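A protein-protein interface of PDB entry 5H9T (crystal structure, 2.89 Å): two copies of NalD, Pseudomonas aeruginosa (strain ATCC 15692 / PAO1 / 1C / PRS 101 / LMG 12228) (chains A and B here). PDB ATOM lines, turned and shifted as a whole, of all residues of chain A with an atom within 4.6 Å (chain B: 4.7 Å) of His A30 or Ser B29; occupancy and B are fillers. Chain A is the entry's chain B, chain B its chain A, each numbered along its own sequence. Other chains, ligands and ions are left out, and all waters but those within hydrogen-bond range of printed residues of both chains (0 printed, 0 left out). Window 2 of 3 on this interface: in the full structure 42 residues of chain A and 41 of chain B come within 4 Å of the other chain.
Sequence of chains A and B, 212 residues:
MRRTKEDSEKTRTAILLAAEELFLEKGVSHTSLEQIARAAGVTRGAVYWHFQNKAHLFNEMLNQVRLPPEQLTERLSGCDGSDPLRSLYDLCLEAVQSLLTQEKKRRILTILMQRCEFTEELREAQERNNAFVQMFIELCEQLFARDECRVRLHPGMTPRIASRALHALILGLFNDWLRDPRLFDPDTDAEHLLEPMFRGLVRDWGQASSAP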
ATOM      1  N   LYS A  26      20.700 -10.421  14.708  1.00  0.00           N
ATOM      2  CA  LYS A  26      20.543 -11.858  14.941  1.00  0.00           C
ATOM      3  C   LYS A  26      20.724 -12.328  16.393  1.00  0.00           C
ATOM      4  O   LYS A  26      20.602 -13.516  16.675  1.00  0.00           O
ATOM      5  CB  LYS A  26      21.513 -12.603  13.976  1.00  0.00           C
ATOM      6  CG  LYS A  26      21.268 -12.551  12.483  1.00  0.00           C
ATOM      7  CD  LYS A  26      22.384 -13.341  11.834  1.00  0.00           C
ATOM      8  CE  LYS A  26      22.246 -13.390  10.325  1.00  0.00           C
ATOM      9  NZ  LYS A  26      23.342 -14.138   9.686  1.00  0.00           N
ATOM     10  N   GLY A  27      21.010 -11.412  17.309  1.00  0.00           N
ATOM     11  CA  GLY A  27      21.224 -11.769  18.712  1.00  0.00           C
ATOM     12  C   GLY A  27      22.680 -12.095  18.998  1.00  0.00           C
ATOM     13  O   GLY A  27      23.428 -12.501  18.102  1.00  0.00           O
ATOM     14  N   VAL A  28      23.088 -11.915  20.250  1.00  0.00           N
ATOM     15  CA  VAL A  28      24.471 -12.155  20.647  1.00  0.00           C
ATOM     16  C   VAL A  28      24.840 -13.634  20.572  1.00  0.00           C
ATOM     17  O   VAL A  28      25.822 -14.006  19.930  1.00  0.00           O
ATOM     18  CB  VAL A  28      24.746 -11.641  22.072  1.00  0.00           C
ATOM     19  CG1 VAL A  28      26.198 -11.885  22.453  1.00  0.00           C
ATOM     20  CG2 VAL A  28      24.401 -10.163  22.179  1.00  0.00           C
ATOM     21  N   SER A  29      24.048 -14.470  21.234  1.00  0.00           N
ATOM     22  CA  SER A  29      24.310 -15.905  21.281  1.00  0.00           C
ATOM     23  C   SER A  29      24.582 -16.492  19.898  1.00  0.00           C
ATOM     24  O   SER A  29      25.501 -17.293  19.725  1.00  0.00           O
ATOM     25  CB  SER A  29      23.140 -16.639  21.940  1.00  0.00           C
ATOM     26  OG  SER A  29      22.691 -15.949  23.093  1.00  0.00           O
ATOM     27  N   HIS A  30      23.778 -16.094  18.917  1.00  0.00           N
ATOM     28  CA  HIS A  30      23.905 -16.627  17.549  1.00  0.00           C
ATOM     29  C   HIS A  30      24.991 -15.915  16.711  1.00  0.00           C
ATOM     30  O   HIS A  30      25.264 -16.315  15.566  1.00  0.00           O
ATOM     31  CB  HIS A  30      22.550 -16.581  16.832  1.00  0.00           C
ATOM     32  CG  HIS A  30      21.549 -17.574  17.350  1.00  0.00           C
ATOM     33  ND1 HIS A  30      21.848 -18.906  17.555  1.00  0.00           N
ATOM     34  CD2 HIS A  30      20.243 -17.429  17.676  1.00  0.00           C
ATOM     35  CE1 HIS A  30      20.772 -19.535  17.996  1.00  0.00           C
ATOM     36  NE2 HIS A  30      19.784 -18.661  18.077  1.00  0.00           N
ATOM     37  N   THR A  31      25.642 -14.913  17.307  1.00  0.00           N
ATOM     38  CA  THR A  31      26.791 -14.232  16.696  1.00  0.00           C
ATOM     39  C   THR A  31      28.119 -14.675  17.320  1.00  0.00           C
ATOM     40  O   THR A  31      28.265 -14.707  18.533  1.00  0.00           O
ATOM     41  CB  THR A  31      26.674 -12.703  16.839  1.00  0.00           C
ATOM     42  OG1 THR A  31      25.431 -12.267  16.284  1.00  0.00           O
ATOM     43  CG2 THR A  31      27.814 -11.989  16.124  1.00  0.00           C
ATOM     44  N   SER A  32      29.085 -14.979  16.465  1.00  0.00           N
ATOM     45  CA  SER A  32      30.404 -15.449  16.880  1.00  0.00           C
ATOM     46  C   SER A  32      31.452 -14.417  16.513  1.00  0.00           C
ATOM     47  O   SER A  32      31.226 -13.570  15.642  1.00  0.00           O
ATOM     48  CB  SER A  32      30.744 -16.750  16.161  1.00  0.00           C
ATOM     49  OG  SER A  32      31.024 -16.507  14.785  1.00  0.00           O
ATOM     50  N   GLN A  35      32.177 -14.559  12.706  1.00  0.00           N
ATOM     51  CA  GLN A  35      31.197 -13.819  11.896  1.00  0.00           C
ATOM     52  C   GLN A  35      31.398 -12.312  11.988  1.00  0.00           C
ATOM     53  O   GLN A  35      31.179 -11.594  11.009  1.00  0.00           O
ATOM     54  CB  GLN A  35      29.779 -14.173  12.324  1.00  0.00           C
ATOM     55  CG  GLN A  35      29.382 -15.580  11.953  1.00  0.00           C
ATOM     56  CD  GLN A  35      28.169 -16.091  12.676  1.00  0.00           C
ATOM     57  OE1 GLN A  35      28.274 -16.215  13.854  1.00  0.00           O
ATOM     58  NE2 GLN A  35      27.030 -16.370  12.015  1.00  0.00           N
ATOM     59  N   GLU A 117      21.083 -12.740  26.089  1.00  0.00           N
ATOM     60  CA  GLU A 117      20.823 -13.615  27.213  1.00  0.00           C
ATOM     61  C   GLU A 117      22.061 -13.706  28.054  1.00  0.00           C
ATOM     62  O   GLU A 117      23.126 -13.893  27.548  1.00  0.00           O
ATOM     63  CB  GLU A 117      20.468 -15.027  26.768  1.00  0.00           C
ATOM     64  CG  GLU A 117      19.931 -15.206  25.368  1.00  0.00           C
ATOM     65  CD  GLU A 117      19.607 -16.651  25.074  1.00  0.00           C
ATOM     66  OE1 GLU A 117      20.175 -17.506  25.728  1.00  0.00           O
ATOM     67  OE2 GLU A 117      18.792 -16.949  24.204  1.00  0.00           O
ATOM     68  N   GLY B  27      19.850 -20.341  28.908  1.00  0.00           N
ATOM     69  CA  GLY B  27      19.331 -19.373  27.944  1.00  0.00           C
ATOM     70  C   GLY B  27      18.519 -20.049  26.873  1.00  0.00           C
ATOM     71  O   GLY B  27      18.742 -21.206  26.563  1.00  0.00           O
ATOM     72  N   VAL B  28      17.594 -19.308  26.288  1.00  0.00           N
ATOM     73  CA  VAL B  28      16.684 -19.837  25.282  1.00  0.00           C
ATOM     74  C   VAL B  28      17.386 -20.123  23.946  1.00  0.00           C
ATOM     75  O   VAL B  28      17.075 -21.113  23.296  1.00  0.00           O
ATOM     76  CB  VAL B  28      15.489 -18.861  25.042  1.00  0.00           C
ATOM     77  CG1 VAL B  28      14.612 -19.297  23.873  1.00  0.00           C
ATOM     78  CG2 VAL B  28      14.643 -18.691  26.306  1.00  0.00           C
ATOM     79  N   SER B  29      18.332 -19.309  23.551  1.00  0.00           N
ATOM     80  CA  SER B  29      18.872 -19.488  22.237  1.00  0.00           C
ATOM     81  C   SER B  29      19.830 -20.639  22.204  1.00  0.00           C
ATOM     82  O   SER B  29      19.998 -21.273  21.184  1.00  0.00           O
ATOM     83  CB  SER B  29      19.546 -18.218  21.770  1.00  0.00           C
ATOM     84  OG  SER B  29      20.760 -18.033  22.452  1.00  0.00           O
ATOM     85  N   HIS B  30      20.473 -20.905  23.321  1.00  0.00           N
ATOM     86  CA  HIS B  30      21.380 -22.048  23.414  1.00  0.00           C
ATOM     87  C   HIS B  30      20.645 -23.347  23.754  1.00  0.00           C
ATOM     88  O   HIS B  30      21.269 -24.417  23.802  1.00  0.00           O
ATOM     89  CB  HIS B  30      22.503 -21.771  24.426  1.00  0.00           C
ATOM     90  CG  HIS B  30      23.515 -20.769  23.954  1.00  0.00           C
ATOM     91  ND1 HIS B  30      24.100 -20.822  22.704  1.00  0.00           N
ATOM     92  CD2 HIS B  30      24.060 -19.698  24.576  1.00  0.00           C
ATOM     93  CE1 HIS B  30      24.953 -19.821  22.577  1.00  0.00           C
ATOM     94  NE2 HIS B  30      24.949 -19.126  23.700  1.00  0.00           N
ATOM     95  N   THR B  31      19.328 -23.248  23.963  1.00  0.00           N
ATOM     96  CA  THR B  31      18.471 -24.407  24.192  1.00  0.00           C
ATOM     97  C   THR B  31      17.676 -24.741  22.937  1.00  0.00           C
ATOM     98  O   THR B  31      17.031 -23.883  22.328  1.00  0.00           O
ATOM     99  CB  THR B  31      17.483 -24.185  25.355  1.00  0.00           C
ATOM    100  OG1 THR B  31      18.216 -23.846  26.539  1.00  0.00           O
ATOM    101  CG2 THR B  31      16.651 -25.434  25.633  1.00  0.00           C
ATOM    102  N   LYS B  54       9.727 -23.295  18.821  1.00  0.00           N
ATOM    103  CA  LYS B  54      10.254 -22.839  20.071  1.00  0.00           C
ATOM    104  C   LYS B  54       9.502 -21.649  20.605  1.00  0.00           C
ATOM    105  O   LYS B  54       9.169 -21.597  21.760  1.00  0.00           O
ATOM    106  CB  LYS B  54      11.706 -22.473  19.875  1.00  0.00           C
ATOM    107  CG  LYS B  54      12.449 -22.180  21.148  1.00  0.00           C
ATOM    108  CD  LYS B  54      13.832 -22.749  21.085  1.00  0.00           C
ATOM    109  CE  LYS B  54      14.855 -21.652  21.081  1.00  0.00           C
ATOM    110  NZ  LYS B  54      16.182 -22.205  20.751  1.00  0.00           N
ATOM    111  N   GLU B 117      16.719 -13.672  24.017  1.00  0.00           N
ATOM    112  CA  GLU B 117      16.919 -12.626  23.020  1.00  0.00           C
ATOM    113  C   GLU B 117      15.740 -12.669  22.092  1.00  0.00           C
ATOM    114  O   GLU B 117      15.351 -13.727  21.658  1.00  0.00           O
ATOM    115  CB  GLU B 117      18.204 -12.854  22.185  1.00  0.00           C
ATOM    116  CG  GLU B 117      19.319 -13.613  22.882  1.00  0.00           C
ATOM    117  CD  GLU B 117      20.532 -13.846  22.017  1.00  0.00           C
ATOM    118  OE1 GLU B 117      21.610 -13.437  22.459  1.00  0.00           O
ATOM    119  OE2 GLU B 117      20.418 -14.429  20.913  1.00  0.00           O
ATOM    120  N   GLU B 121      13.696 -15.753  15.477  1.00  0.00           N
ATOM    121  CA  GLU B 121      13.288 -17.050  16.009  1.00  0.00           C
ATOM    122  C   GLU B 121      12.141 -16.941  17.019  1.00  0.00           C
ATOM    123  O   GLU B 121      11.306 -17.825  17.092  1.00  0.00           O
ATOM    124  CB  GLU B 121      14.492 -17.763  16.649  1.00  0.00           C
ATOM    125  CG  GLU B 121      14.207 -19.200  17.080  1.00  0.00           C
ATOM    126  CD  GLU B 121      15.437 -20.002  17.521  1.00  0.00           C
ATOM    127  OE1 GLU B 121      15.704 -21.085  16.944  1.00  0.00           O
ATOM    128  OE2 GLU B 121      16.130 -19.578  18.468  1.00  0.00           O
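The backbone NH of Val B28 is in hydrogen-bond range of the side-chain carboxylate of Glu A117 (3.2 Å).
The side-chain hydroxyl (OG) of Ser B29 lies close to the side-chain hydroxyl (OG) of Ser A29, 2.9 Å away.
The side-chain carboxylate (OE2) of Glu A117 sits at hydrogen-bond distance from the backbone NH (N) of Ser B29, 2.5 Å away.
OE1 of Glu B117 sits at hydrogen-bond distance from N of Val A28, at 3.1 Å.
The side-chain carboxylate of Glu B117 is in hydrogen-bond range of the side-chain hydroxyl of Ser A29, at 2.8 Å.
OG1 of Thr B31 sits at hydrogen-bond distance from O of Gly B27 (2.7 Å).
The backbone carbonyl oxygen (O) of Val B28 is in hydrogen-bond range of the side-chain amino group (NZ) of Lys B54, at 2.9 Å.
The side-chain carboxylate (OE2) of Glu B121 lies within salt-bridge range of the side-chain amino group (NZ) of Lys B54 (3.5 Å).
The backbone carbonyl oxygen (O) of Gly A27 lies within hydrogen-bond range of the side-chain hydroxyl (OG1) of Thr A31, 2.7 Å away.
O of His A30 sits close to OE1 of Gln A35.
Among the printed residues, pairs that only touch across the chains: Gly A27 with Glu B117, Ser A29 with His B30, His A30 with Ser B29, His A30 with Glu B121, Glu A117 with Gly B27 and Glu A117 with Glu B117.
Of the printed residues of chain A, Ser B29 touches Ser A29, His A30 and Glu A117.
Of the printed residues of chain B, Gly A27 touches Glu B117.
Of the printed residues of chain B, Ser A29 touches Ser B29 (2.8 Å), His B30 (3.5 Å) and Glu B117 (2.8 Å).
Thr B31 touches none of the printed residues of chain A.
Of the 9 printed residues of chain A, 5 touch a printed residue of chain B.
Hydrophobic or aromatic side chains of chain A that line the printed part of chain B: Val A28 and His A30.
Of the 8 printed residues of chain B, 6 touch a printed residue of chain A.
Hydrophobic or aromatic side chains of chain B that line the printed part of chain A: Val B28 and His B30.
Ser A29 touches its own counterpart, Ser B29.
Ser A29 touches His B30, and with the chains exchanged His A30 touches Ser B29.
Ser A29 touches Glu B117, and with the chains exchanged Glu A117 touches Ser B29.
Glu A117 touches its own counterpart, Glu B117.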
